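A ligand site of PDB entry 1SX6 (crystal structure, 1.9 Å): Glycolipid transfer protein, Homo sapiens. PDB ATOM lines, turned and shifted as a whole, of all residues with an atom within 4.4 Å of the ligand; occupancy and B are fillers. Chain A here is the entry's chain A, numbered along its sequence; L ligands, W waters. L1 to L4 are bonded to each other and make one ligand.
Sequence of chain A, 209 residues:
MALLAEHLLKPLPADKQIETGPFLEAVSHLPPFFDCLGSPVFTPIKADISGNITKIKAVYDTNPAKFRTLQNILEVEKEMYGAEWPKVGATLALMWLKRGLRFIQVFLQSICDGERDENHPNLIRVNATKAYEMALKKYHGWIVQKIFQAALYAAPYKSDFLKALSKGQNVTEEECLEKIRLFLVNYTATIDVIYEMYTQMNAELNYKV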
ATOM      1  N   LEU A   4      25.110 -14.896  -4.493  1.00  0.00           N
ATOM      2  CA  LEU A   4      25.247 -16.290  -5.030  1.00  0.00           C
ATOM      3  C   LEU A   4      26.290 -17.101  -4.263  1.00  0.00           C
ATOM      4  O   LEU A   4      26.039 -18.250  -3.887  1.00  0.00           O
ATOM      5  CB  LEU A   4      25.619 -16.269  -6.514  1.00  0.00           C
ATOM      6  CG  LEU A   4      25.889 -17.622  -7.195  1.00  0.00           C
ATOM      7  CD1 LEU A   4      24.729 -18.599  -7.007  1.00  0.00           C
ATOM      8  CD2 LEU A   4      26.175 -17.409  -8.670  1.00  0.00           C
ATOM      9  N   LEU A  30      18.010 -20.403  -5.166  1.00  0.00           N
ATOM     10  CA  LEU A  30      18.190 -20.351  -6.624  1.00  0.00           C
ATOM     11  C   LEU A  30      16.979 -19.810  -7.400  1.00  0.00           C
ATOM     12  O   LEU A  30      17.165 -18.981  -8.264  1.00  0.00           O
ATOM     13  CB  LEU A  30      18.662 -21.702  -7.205  1.00  0.00           C
ATOM     14  CG  LEU A  30      19.980 -22.234  -6.630  1.00  0.00           C
ATOM     15  CD1 LEU A  30      20.228 -23.697  -6.987  1.00  0.00           C
ATOM     16  CD2 LEU A  30      21.161 -21.383  -7.070  1.00  0.00           C
ATOM     17  N   PHE A  33      16.531 -15.979  -8.437  1.00  0.00           N
ATOM     18  CA  PHE A  33      17.344 -15.504  -9.581  1.00  0.00           C
ATOM     19  C   PHE A  33      16.582 -15.495 -10.936  1.00  0.00           C
ATOM     20  O   PHE A  33      16.999 -14.820 -11.877  1.00  0.00           O
ATOM     21  CB  PHE A  33      18.626 -16.327  -9.723  1.00  0.00           C
ATOM     22  CG  PHE A  33      19.667 -16.035  -8.662  1.00  0.00           C
ATOM     23  CD1 PHE A  33      19.793 -16.845  -7.539  1.00  0.00           C
ATOM     24  CD2 PHE A  33      20.525 -14.942  -8.790  1.00  0.00           C
ATOM     25  CE1 PHE A  33      20.742 -16.579  -6.562  1.00  0.00           C
ATOM     26  CE2 PHE A  33      21.491 -14.663  -7.819  1.00  0.00           C
ATOM     27  CZ  PHE A  33      21.596 -15.478  -6.700  1.00  0.00           C
ATOM     28  N   PHE A  34      15.485 -16.253 -11.022  1.00  0.00           N
ATOM     29  CA  PHE A  34      14.665 -16.277 -12.236  1.00  0.00           C
ATOM     30  C   PHE A  34      13.818 -15.024 -12.444  1.00  0.00           C
ATOM     31  O   PHE A  34      13.462 -14.705 -13.579  1.00  0.00           O
ATOM     32  CB  PHE A  34      13.757 -17.506 -12.254  1.00  0.00           C
ATOM     33  CG  PHE A  34      14.485 -18.762 -12.558  1.00  0.00           C
ATOM     34  CD1 PHE A  34      14.957 -19.000 -13.852  1.00  0.00           C
ATOM     35  CD2 PHE A  34      14.751 -19.695 -11.575  1.00  0.00           C
ATOM     36  CE1 PHE A  34      15.642 -20.146 -14.147  1.00  0.00           C
ATOM     37  CE2 PHE A  34      15.455 -20.850 -11.865  1.00  0.00           C
ATOM     38  CZ  PHE A  34      15.889 -21.078 -13.148  1.00  0.00           C
ATOM     39  N   LEU A  37      15.802 -12.350 -14.765  1.00  0.00           N
ATOM     40  CA  LEU A  37      16.261 -12.664 -16.124  1.00  0.00           C
ATOM     41  C   LEU A  37      15.499 -11.803 -17.133  1.00  0.00           C
ATOM     42  O   LEU A  37      15.845 -11.798 -18.325  1.00  0.00           O
ATOM     43  CB  LEU A  37      16.047 -14.146 -16.448  1.00  0.00           C
ATOM     44  CG  LEU A  37      17.279 -15.039 -16.344  1.00  0.00           C
ATOM     45  CD1 LEU A  37      17.792 -15.042 -14.926  1.00  0.00           C
ATOM     46  CD2 LEU A  37      16.936 -16.444 -16.802  1.00  0.00           C
ATOM     47  N   PHE A  42       9.992 -17.076 -17.724  1.00  0.00           N
ATOM     48  CA  PHE A  42      10.684 -17.833 -16.691  1.00  0.00           C
ATOM     49  C   PHE A  42       9.818 -18.170 -15.489  1.00  0.00           C
ATOM     50  O   PHE A  42      10.232 -18.928 -14.636  1.00  0.00           O
ATOM     51  CB  PHE A  42      11.945 -17.095 -16.258  1.00  0.00           C
ATOM     52  CG  PHE A  42      12.917 -16.917 -17.383  1.00  0.00           C
ATOM     53  CD1 PHE A  42      13.585 -18.016 -17.897  1.00  0.00           C
ATOM     54  CD2 PHE A  42      13.123 -15.676 -17.966  1.00  0.00           C
ATOM     55  CE1 PHE A  42      14.445 -17.879 -18.967  1.00  0.00           C
ATOM     56  CE2 PHE A  42      13.998 -15.527 -19.032  1.00  0.00           C
ATOM     57  CZ  PHE A  42      14.657 -16.631 -19.538  1.00  0.00           C
ATOM     58  N   ILE A  45       9.093 -21.797 -15.176  1.00  0.00           N
ATOM     59  CA  ILE A  45      10.364 -22.448 -14.930  1.00  0.00           C
ATOM     60  C   ILE A  45      10.687 -22.407 -13.434  1.00  0.00           C
ATOM     61  O   ILE A  45      11.028 -23.433 -12.834  1.00  0.00           O
ATOM     62  CB  ILE A  45      11.465 -21.761 -15.738  1.00  0.00           C
ATOM     63  CG1 ILE A  45      11.241 -22.072 -17.230  1.00  0.00           C
ATOM     64  CG2 ILE A  45      12.866 -22.221 -15.267  1.00  0.00           C
ATOM     65  CD1 ILE A  45      12.076 -21.254 -18.185  1.00  0.00           C
ATOM     66  N   ASP A  48       8.460 -24.778 -11.480  1.00  0.00           N
ATOM     67  CA  ASP A  48       8.756 -26.207 -11.538  1.00  0.00           C
ATOM     68  C   ASP A  48       9.833 -26.529 -10.486  1.00  0.00           C
ATOM     69  O   ASP A  48       9.704 -27.502  -9.732  1.00  0.00           O
ATOM     70  CB  ASP A  48       9.209 -26.627 -12.939  1.00  0.00           C
ATOM     71  CG  ASP A  48       9.635 -28.089 -12.975  1.00  0.00           C
ATOM     72  OD1 ASP A  48       8.793 -28.942 -13.338  1.00  0.00           O
ATOM     73  OD2 ASP A  48      10.763 -28.467 -12.611  1.00  0.00           O
ATOM     74  N   ASN A  52       9.181 -28.463  -6.902  1.00  0.00           N
ATOM     75  CA  ASN A  52       9.862 -29.698  -6.518  1.00  0.00           C
ATOM     76  C   ASN A  52      10.555 -29.594  -5.170  1.00  0.00           C
ATOM     77  O   ASN A  52      10.463 -30.515  -4.366  1.00  0.00           O
ATOM     78  CB  ASN A  52      10.807 -30.143  -7.637  1.00  0.00           C
ATOM     79  CG  ASN A  52      10.054 -30.791  -8.782  1.00  0.00           C
ATOM     80  OD1 ASN A  52       9.113 -31.553  -8.552  1.00  0.00           O
ATOM     81  ND2 ASN A  52      10.449 -30.492 -10.015  1.00  0.00           N
ATOM     82  N   LYS A  55       7.875 -29.851  -2.552  1.00  0.00           N
ATOM     83  CA  LYS A  55       7.405 -31.232  -2.443  1.00  0.00           C
ATOM     84  C   LYS A  55       8.372 -32.094  -1.622  1.00  0.00           C
ATOM     85  O   LYS A  55       7.920 -32.886  -0.791  1.00  0.00           O
ATOM     86  CB  LYS A  55       7.149 -31.840  -3.850  1.00  0.00           C
ATOM     87  CG  LYS A  55       5.792 -31.382  -4.444  1.00  0.00           C
ATOM     88  CD  LYS A  55       5.773 -31.263  -5.992  1.00  0.00           C
ATOM     89  CE  LYS A  55       4.423 -30.693  -6.513  1.00  0.00           C
ATOM     90  NZ  LYS A  55       4.341 -30.626  -8.003  1.00  0.00           N
ATOM     91  N   LEU A  92      10.440 -38.719  -6.870  1.00  0.00           N
ATOM     92  CA  LEU A  92      10.106 -38.222  -8.186  1.00  0.00           C
ATOM     93  C   LEU A  92      10.358 -36.716  -8.285  1.00  0.00           C
ATOM     94  O   LEU A  92      10.909 -36.228  -9.276  1.00  0.00           O
ATOM     95  CB  LEU A  92       8.665 -38.527  -8.530  1.00  0.00           C
ATOM     96  CG  LEU A  92       8.171 -38.136  -9.915  1.00  0.00           C
ATOM     97  CD1 LEU A  92       9.106 -38.666 -11.026  1.00  0.00           C
ATOM     98  CD2 LEU A  92       6.770 -38.675 -10.084  1.00  0.00           C
ATOM     99  N   ALA A  93       9.955 -35.975  -7.243  1.00  0.00           N
ATOM    100  CA  ALA A  93      10.257 -34.554  -7.187  1.00  0.00           C
ATOM    101  C   ALA A  93      11.755 -34.294  -7.374  1.00  0.00           C
ATOM    102  O   ALA A  93      12.138 -33.447  -8.169  1.00  0.00           O
ATOM    103  CB  ALA A  93       9.801 -33.955  -5.859  1.00  0.00           C
ATOM    104  N   TRP A  96      13.292 -34.777 -10.911  1.00  0.00           N
ATOM    105  CA  TRP A  96      13.152 -33.609 -11.751  1.00  0.00           C
ATOM    106  C   TRP A  96      13.919 -32.384 -11.243  1.00  0.00           C
ATOM    107  O   TRP A  96      14.386 -31.573 -12.039  1.00  0.00           O
ATOM    108  CB  TRP A  96      11.666 -33.296 -11.954  1.00  0.00           C
ATOM    109  CG  TRP A  96      11.026 -34.263 -12.865  1.00  0.00           C
ATOM    110  CD1 TRP A  96      10.338 -35.360 -12.532  1.00  0.00           C
ATOM    111  CD2 TRP A  96      11.094 -34.245 -14.299  1.00  0.00           C
ATOM    112  NE1 TRP A  96       9.935 -36.031 -13.655  1.00  0.00           N
ATOM    113  CE2 TRP A  96      10.375 -35.355 -14.755  1.00  0.00           C
ATOM    114  CE3 TRP A  96      11.665 -33.390 -15.235  1.00  0.00           C
ATOM    115  CZ2 TRP A  96      10.215 -35.638 -16.108  1.00  0.00           C
ATOM    116  CZ3 TRP A  96      11.503 -33.660 -16.578  1.00  0.00           C
ATOM    117  CH2 TRP A  96      10.791 -34.771 -17.002  1.00  0.00           C
ATOM    118  N   GLY A 100      16.791 -29.953 -13.248  1.00  0.00           N
ATOM    119  CA  GLY A 100      16.767 -28.513 -13.135  1.00  0.00           C
ATOM    120  C   GLY A 100      18.060 -27.906 -12.642  1.00  0.00           C
ATOM    121  O   GLY A 100      18.581 -26.975 -13.251  1.00  0.00           O
ATOM    122  N   PHE A 103      20.844 -28.441 -15.130  1.00  0.00           N
ATOM    123  CA  PHE A 103      20.759 -27.472 -16.213  1.00  0.00           C
ATOM    124  C   PHE A 103      21.459 -26.176 -15.793  1.00  0.00           C
ATOM    125  O   PHE A 103      22.194 -25.601 -16.576  1.00  0.00           O
ATOM    126  CB  PHE A 103      19.318 -27.188 -16.611  1.00  0.00           C
ATOM    127  CG  PHE A 103      19.199 -26.075 -17.621  1.00  0.00           C
ATOM    128  CD1 PHE A 103      19.032 -26.359 -18.945  1.00  0.00           C
ATOM    129  CD2 PHE A 103      19.316 -24.736 -17.218  1.00  0.00           C
ATOM    130  CE1 PHE A 103      18.939 -25.342 -19.887  1.00  0.00           C
ATOM    131  CE2 PHE A 103      19.236 -23.706 -18.146  1.00  0.00           C
ATOM    132  CZ  PHE A 103      19.043 -24.015 -19.497  1.00  0.00           C
ATOM    133  N   ILE A 104      21.200 -25.713 -14.572  1.00  0.00           N
ATOM    134  CA  ILE A 104      21.826 -24.497 -14.056  1.00  0.00           C
ATOM    135  C   ILE A 104      23.355 -24.684 -13.987  1.00  0.00           C
ATOM    136  O   ILE A 104      24.127 -23.785 -14.350  1.00  0.00           O
ATOM    137  CB  ILE A 104      21.233 -24.157 -12.678  1.00  0.00           C
ATOM    138  CG1 ILE A 104      19.774 -23.725 -12.854  1.00  0.00           C
ATOM    139  CG2 ILE A 104      22.051 -23.060 -11.971  1.00  0.00           C
ATOM    140  CD1 ILE A 104      19.014 -23.569 -11.577  1.00  0.00           C
ATOM    141  N   PHE A 107      24.840 -24.714 -17.662  1.00  0.00           N
ATOM    142  CA  PHE A 107      24.731 -23.362 -18.166  1.00  0.00           C
ATOM    143  C   PHE A 107      25.819 -22.448 -17.590  1.00  0.00           C
ATOM    144  O   PHE A 107      26.571 -21.783 -18.317  1.00  0.00           O
ATOM    145  CB  PHE A 107      23.358 -22.833 -17.819  1.00  0.00           C
ATOM    146  CG  PHE A 107      23.127 -21.422 -18.250  1.00  0.00           C
ATOM    147  CD1 PHE A 107      23.115 -21.101 -19.601  1.00  0.00           C
ATOM    148  CD2 PHE A 107      22.933 -20.413 -17.313  1.00  0.00           C
ATOM    149  CE1 PHE A 107      22.893 -19.797 -20.019  1.00  0.00           C
ATOM    150  CE2 PHE A 107      22.707 -19.124 -17.722  1.00  0.00           C
ATOM    151  CZ  PHE A 107      22.692 -18.809 -19.094  1.00  0.00           C
ATOM    152  N   LEU A 108      25.914 -22.421 -16.272  1.00  0.00           N
ATOM    153  CA  LEU A 108      26.889 -21.563 -15.640  1.00  0.00           C
ATOM    154  C   LEU A 108      28.328 -21.956 -15.972  1.00  0.00           C
ATOM    155  O   LEU A 108      29.153 -21.086 -16.169  1.00  0.00           O
ATOM    156  CB  LEU A 108      26.671 -21.492 -14.130  1.00  0.00           C
ATOM    157  CG  LEU A 108      25.361 -20.849 -13.665  1.00  0.00           C
ATOM    158  CD1 LEU A 108      25.248 -20.936 -12.128  1.00  0.00           C
ATOM    159  CD2 LEU A 108      25.243 -19.405 -14.130  1.00  0.00           C
ATOM    160  N   ALA A 128      22.941 -21.952 -23.023  1.00  0.00           N
ATOM    161  CA  ALA A 128      21.646 -22.474 -22.622  1.00  0.00           C
ATOM    162  C   ALA A 128      21.247 -23.704 -23.422  1.00  0.00           C
ATOM    163  O   ALA A 128      20.610 -24.603 -22.893  1.00  0.00           O
ATOM    164  CB  ALA A 128      20.580 -21.381 -22.737  1.00  0.00           C
ATOM    165  N   LEU A 136      18.132 -31.803 -19.881  1.00  0.00           N
ATOM    166  CA  LEU A 136      16.696 -31.850 -19.999  1.00  0.00           C
ATOM    167  C   LEU A 136      16.114 -32.497 -21.246  1.00  0.00           C
ATOM    168  O   LEU A 136      15.098 -33.151 -21.148  1.00  0.00           O
ATOM    169  CB  LEU A 136      16.132 -30.441 -19.923  1.00  0.00           C
ATOM    170  CG  LEU A 136      16.219 -29.711 -18.589  1.00  0.00           C
ATOM    171  CD1 LEU A 136      15.737 -28.290 -18.792  1.00  0.00           C
ATOM    172  CD2 LEU A 136      15.387 -30.389 -17.531  1.00  0.00           C
ATOM    173  N   HIS A 140      12.139 -34.583 -22.819  1.00  0.00           N
ATOM    174  CA  HIS A 140      11.100 -33.741 -23.380  1.00  0.00           C
ATOM    175  C   HIS A 140      10.642 -34.283 -24.742  1.00  0.00           C
ATOM    176  O   HIS A 140      11.471 -34.587 -25.601  1.00  0.00           O
ATOM    177  CB  HIS A 140      11.619 -32.320 -23.559  1.00  0.00           C
ATOM    178  CG  HIS A 140      11.789 -31.596 -22.266  1.00  0.00           C
ATOM    179  ND1 HIS A 140      12.069 -30.244 -22.204  1.00  0.00           N
ATOM    180  CD2 HIS A 140      11.705 -32.022 -20.979  1.00  0.00           C
ATOM    181  CE1 HIS A 140      12.133 -29.873 -20.936  1.00  0.00           C
ATOM    182  NE2 HIS A 140      11.914 -30.931 -20.172  1.00  0.00           N
ATOM    183  N   PHE A 148      10.882 -24.766 -25.513  1.00  0.00           N
ATOM    184  CA  PHE A 148      12.220 -24.332 -25.090  1.00  0.00           C
ATOM    185  C   PHE A 148      12.847 -23.382 -26.106  1.00  0.00           C
ATOM    186  O   PHE A 148      13.381 -22.340 -25.756  1.00  0.00           O
ATOM    187  CB  PHE A 148      13.167 -25.509 -24.910  1.00  0.00           C
ATOM    188  CG  PHE A 148      14.635 -25.087 -24.879  1.00  0.00           C
ATOM    189  CD1 PHE A 148      15.158 -24.447 -23.748  1.00  0.00           C
ATOM    190  CD2 PHE A 148      15.474 -25.289 -25.983  1.00  0.00           C
ATOM    191  CE1 PHE A 148      16.490 -24.042 -23.708  1.00  0.00           C
ATOM    192  CE2 PHE A 148      16.805 -24.898 -25.943  1.00  0.00           C
ATOM    193  CZ  PHE A 148      17.322 -24.272 -24.793  1.00  0.00           C
ATOM    194  N   ALA A 151      11.307 -20.056 -25.789  1.00  0.00           N
ATOM    195  CA  ALA A 151      11.715 -19.480 -24.510  1.00  0.00           C
ATOM    196  C   ALA A 151      13.152 -18.991 -24.538  1.00  0.00           C
ATOM    197  O   ALA A 151      13.511 -18.090 -23.787  1.00  0.00           O
ATOM    198  CB  ALA A 151      11.534 -20.513 -23.377  1.00  0.00           C
ATOM    199  N   ALA A 155      16.111 -15.068 -23.226  1.00  0.00           N
ATOM    200  CA  ALA A 155      17.467 -14.937 -22.686  1.00  0.00           C
ATOM    201  C   ALA A 155      18.063 -13.542 -22.918  1.00  0.00           C
ATOM    202  O   ALA A 155      18.044 -13.054 -24.056  1.00  0.00           O
ATOM    203  CB  ALA A 155      18.384 -15.969 -23.295  1.00  0.00           C
ATOM    204  N   PHE A 161      23.106 -10.402 -18.019  1.00  0.00           N
ATOM    205  CA  PHE A 161      22.824 -11.528 -17.137  1.00  0.00           C
ATOM    206  C   PHE A 161      23.789 -11.523 -15.959  1.00  0.00           C
ATOM    207  O   PHE A 161      23.392 -11.792 -14.829  1.00  0.00           O
ATOM    208  CB  PHE A 161      22.975 -12.841 -17.918  1.00  0.00           C
ATOM    209  CG  PHE A 161      22.875 -14.074 -17.073  1.00  0.00           C
ATOM    210  CD1 PHE A 161      21.665 -14.422 -16.478  1.00  0.00           C
ATOM    211  CD2 PHE A 161      23.981 -14.895 -16.877  1.00  0.00           C
ATOM    212  CE1 PHE A 161      21.561 -15.562 -15.676  1.00  0.00           C
ATOM    213  CE2 PHE A 161      23.880 -16.035 -16.085  1.00  0.00           C
ATOM    214  CZ  PHE A 161      22.671 -16.368 -15.489  1.00  0.00           C
ATOM    215  N   LEU A 165      23.284 -10.703 -11.877  1.00  0.00           N
ATOM    216  CA  LEU A 165      23.733 -11.525 -10.769  1.00  0.00           C
ATOM    217  C   LEU A 165      24.509 -10.699  -9.743  1.00  0.00           C
ATOM    218  O   LEU A 165      24.551 -11.070  -8.569  1.00  0.00           O
ATOM    219  CB  LEU A 165      24.591 -12.690 -11.279  1.00  0.00           C
ATOM    220  CG  LEU A 165      23.863 -13.793 -12.056  1.00  0.00           C
ATOM    221  CD1 LEU A 165      24.852 -14.674 -12.792  1.00  0.00           C
ATOM    222  CD2 LEU A 165      23.007 -14.623 -11.137  1.00  0.00           C
ATOM    223  N   TYR A 207      11.125 -41.567 -18.891  1.00  0.00           N
ATOM    224  CA  TYR A 207       9.913 -41.141 -19.584  1.00  0.00           C
ATOM    225  C   TYR A 207       9.992 -39.657 -20.003  1.00  0.00           C
ATOM    226  O   TYR A 207      10.634 -38.842 -19.338  1.00  0.00           O
ATOM    227  CB  TYR A 207       8.670 -41.426 -18.740  1.00  0.00           C
ATOM    228  CG  TYR A 207       8.441 -40.467 -17.585  1.00  0.00           C
ATOM    229  CD1 TYR A 207       7.649 -39.340 -17.728  1.00  0.00           C
ATOM    230  CD2 TYR A 207       9.004 -40.713 -16.338  1.00  0.00           C
ATOM    231  CE1 TYR A 207       7.441 -38.460 -16.660  1.00  0.00           C
ATOM    232  CE2 TYR A 207       8.801 -39.826 -15.259  1.00  0.00           C
ATOM    233  CZ  TYR A 207       8.022 -38.707 -15.430  1.00  0.00           C
ATOM    234  OH  TYR A 207       7.807 -37.833 -14.364  1.00  0.00           O
ATOM    235  N   VAL A 209       7.912 -36.017 -21.338  1.00  0.00           N
ATOM    236  CA  VAL A 209       6.740 -35.220 -21.057  1.00  0.00           C
ATOM    237  C   VAL A 209       6.344 -34.343 -22.245  1.00  0.00           C
ATOM    238  O   VAL A 209       7.131 -33.921 -23.086  1.00  0.00           O
ATOM    239  CB  VAL A 209       6.905 -34.311 -19.797  1.00  0.00           C
ATOM    240  CG1 VAL A 209       7.160 -35.162 -18.560  1.00  0.00           C
ATOM    241  CG2 VAL A 209       8.012 -33.287 -19.988  1.00  0.00           C
ATOM    242  OXT VAL A 209       5.180 -33.980 -22.402  1.00  0.00           O
HETATM  243  C1  LIG L   1       5.165 -35.242  -9.886  1.00  0.00           C
HETATM  244  C2  LIG L   1       4.858 -34.176  -8.853  1.00  0.00           C
HETATM  245  C3  LIG L   1       3.587 -34.564  -8.076  1.00  0.00           C
HETATM  246  C4  LIG L   1       2.479 -34.958  -9.050  1.00  0.00           C
HETATM  247  C5  LIG L   1       2.987 -35.985 -10.055  1.00  0.00           C
HETATM  248  C6  LIG L   1       1.933 -36.461 -11.067  1.00  0.00           C
HETATM  249  O1  LIG L   1       6.006 -34.081  -8.033  1.00  0.00           O
HETATM  250  O2  LIG L   1       3.172 -33.549  -7.192  1.00  0.00           O
HETATM  251  O3  LIG L   1       2.056 -33.810  -9.752  1.00  0.00           O
HETATM  252  O4  LIG L   1       4.061 -35.404 -10.757  1.00  0.00           O
HETATM  253  O5  LIG L   1       1.895 -37.884 -11.102  1.00  0.00           O
HETATM  254  C1  LG2 L   2       7.552 -31.829 -12.185  1.00  0.00           C
HETATM  255  C2  LG2 L   2       7.457 -32.945 -11.165  1.00  0.00           C
HETATM  256  C3  LG2 L   2       6.344 -33.917 -11.541  1.00  0.00           C
HETATM  257  C4  LG2 L   2       6.616 -34.542 -12.903  1.00  0.00           C
HETATM  258  C5  LG2 L   2       5.525 -35.535 -13.346  1.00  0.00           C
HETATM  259  C6  LG2 L   2       7.074 -32.205 -13.615  1.00  0.00           C
HETATM  260  O1  LG2 L   2       7.935 -31.701 -14.613  1.00  0.00           O
HETATM  261  O2  LG2 L   2       8.812 -31.228 -12.101  1.00  0.00           O
HETATM  262  O3  LG2 L   2       7.174 -32.374  -9.898  1.00  0.00           O
HETATM  263  O4  LG2 L   2       6.351 -34.920 -10.569  1.00  0.00           O
HETATM  264  O5  LG2 L   2       6.821 -33.570 -13.917  1.00  0.00           O
HETATM  265  O6  LG2 L   2       5.931 -36.174 -14.542  1.00  0.00           O
HETATM  266  C1  LG3 L   3       8.275 -31.979 -15.888  1.00  0.00           C
HETATM  267  C2  LG3 L   3       8.825 -30.784 -16.676  1.00  0.00           C
HETATM  268  N1  LG3 L   3       9.961 -30.232 -15.943  1.00  0.00           N
HETATM  269  C3  LG3 L   3       7.767 -29.697 -16.913  1.00  0.00           C
HETATM  270  O1  LG3 L   3       6.678 -30.246 -17.625  1.00  0.00           O
HETATM  271  C4  LG3 L   3       8.324 -28.532 -17.679  1.00  0.00           C
HETATM  272  C5  LG3 L   3       8.617 -27.255 -16.997  1.00  0.00           C
HETATM  273  C6  LG3 L   3       9.149 -26.060 -17.768  1.00  0.00           C
HETATM  274  C7  LG3 L   3      10.495 -26.390 -18.452  1.00  0.00           C
HETATM  275  C8  LG3 L   3      10.573 -25.939 -19.916  1.00  0.00           C
HETATM  276  C9  LG3 L   3      12.002 -25.944 -20.489  1.00  0.00           C
HETATM  277  C10 LG3 L   3      12.363 -24.643 -21.209  1.00  0.00           C
HETATM  278  C11 LG3 L   3      13.550 -23.923 -20.567  1.00  0.00           C
HETATM  279  C12 LG3 L   3      13.731 -22.482 -21.095  1.00  0.00           C
HETATM  280  C13 LG3 L   3      14.880 -21.803 -20.370  1.00  0.00           C
HETATM  281  C14 LG3 L   3      15.827 -21.017 -21.287  1.00  0.00           C
HETATM  282  C15 LG3 L   3      17.020 -20.564 -20.437  1.00  0.00           C
HETATM  283  C16 LG3 L   3      17.850 -19.432 -21.044  1.00  0.00           C
HETATM  284  C17 LG3 L   3      18.091 -18.269 -20.066  1.00  0.00           C
HETATM  285  C18 LG3 L   3      19.166 -18.554 -19.025  1.00  0.00           C
HETATM  286  C1  LG4 L   4      11.219 -30.040 -16.002  1.00  0.00           C
HETATM  287  O1  LG4 L   4      11.671 -30.404 -17.322  1.00  0.00           O
HETATM  288  C2  LG4 L   4      12.386 -29.384 -15.272  1.00  0.00           C
HETATM  289  C3  LG4 L   4      12.418 -27.904 -15.651  1.00  0.00           C
HETATM  290  C4  LG4 L   4      13.772 -27.271 -15.401  1.00  0.00           C
HETATM  291  C5  LG4 L   4      14.003 -26.041 -16.275  1.00  0.00           C
HETATM  292  C6  LG4 L   4      15.385 -25.452 -16.039  1.00  0.00           C
HETATM  293  C7  LG4 L   4      15.601 -24.242 -16.948  1.00  0.00           C
HETATM  294  C8  LG4 L   4      16.304 -23.121 -16.177  1.00  0.00           C
HETATM  295  C9  LG4 L   4      16.490 -21.909 -17.083  1.00  0.00           C
HETATM  296  C10 LG4 L   4      17.565 -20.924 -16.881  1.00  0.00           C
HETATM  297  C11 LG4 L   4      18.591 -21.023 -15.750  1.00  0.00           C
HETATM  298  C12 LG4 L   4      19.289 -19.680 -15.546  1.00  0.00           C
HETATM  299  C13 LG4 L   4      20.121 -19.672 -14.267  1.00  0.00           C
HETATM  300  C14 LG4 L   4      19.362 -18.995 -13.136  1.00  0.00           C
HETATM  301  C15 LG4 L   4      19.926 -19.384 -11.765  1.00  0.00           C
HETATM  302  C16 LG4 L   4      21.167 -18.557 -11.460  1.00  0.00           C
HETATM  303  C17 LG4 L   4      21.847 -19.097 -10.205  1.00  0.00           C
HETATM  304  C18 LG4 L   4      23.125 -18.344  -9.902  1.00  0.00           C
HETATM  305  O   HOH W   1       3.562 -31.640 -11.394  1.00  0.00           O
HETATM  306  O   HOH W   2       2.462 -34.778  -4.808  1.00  0.00           O
HETATM  307  O   HOH W   3       6.050 -36.305  -6.790  1.00  0.00           O
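The side-chain amide oxygen (OD1) of Asn 52 lies within hydrogen-bond range of an oxygen (O3) of LG2 L2 (2.5 Å).
OH of Tyr 207 lies within hydrogen-bond range of O6 of LG2 L2 (2.5 Å).
O2 of LG2 L2 lies within hydrogen-bond range of OD1 of Asp 48, 2.6 Å away.
An oxygen (O1) of LG4 L4 sits at hydrogen-bond distance from a ring nitrogen (NE2) of His 140 (2.9 Å).
The side-chain amino group (NZ) of Lys 55 sits close to an oxygen (O2) of LIG L1 (3.3 Å).
ND2 of Asn 52 is in hydrogen-bond range of O of Asp 48 (3.1 Å).
OH of Tyr 207 lies within hydrogen-bond range of NE1 of Trp 96 (2.9 Å).
Leu 4 touches the ligand.
CD2 of Leu 30 touches C17 of LG4 L4, at 3.9 Å.
Phe 33 touches the ligand.
Phe 34 touches the ligand.
CD2 of Leu 37 touches C18 of LG3 L3 (3.8 Å).
CE1 of Phe 42 touches C17 of LG3 L3, at 3.8 Å.
CD1 of Ile 45 touches C12 of LG3 L3, at 3.6 Å.
CG of Leu 92 touches O4 of LG2 L2 (3.8 Å).
CZ3 of Trp 96 touches O1 of LG4 L4, at 3.3 Å.
Gly 100 touches the ligand.
Phe 103 touches the ligand.
Phe 107 touches the ligand.
CB of Ala 128 touches C16 of LG3 L3, 3.8 Å away.
Leu 136 touches the ligand.
CD1 of Phe 148 touches C12 of LG3 L3 (3.6 Å).
Ala 151 touches the ligand.
Ala 155 touches the ligand.
CD2 of Leu 165 touches C18 of LG4 L4, 3.9 Å away.
Hydrophobic or aromatic side chains that line the ligand: Leu 4, Leu 30, Phe 33, Phe 34, Leu 37, Phe 42, Ile 45, Leu 92, Trp 96, Phe 103, Phe 107, Ala 128, Leu 136, His 140, Phe 148, Ala 151, Ala 155, Leu 165 and Tyr 207.
Within 4 Å of the ligand: Leu 4, Leu 30, Phe 33, Phe 34, Leu 37, Phe 42, Ile 45, Asp 48, Asn 52, Lys 55, Leu 92, Trp 96, Gly 100, Phe 103, Phe 107, Ala 128, Leu 136, His 140, Phe 148, Ala 151, Ala 155, Leu 165 and Tyr 207.
The nearest printed residue that does not touch the ligand is Leu 108 (4.02 Å).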
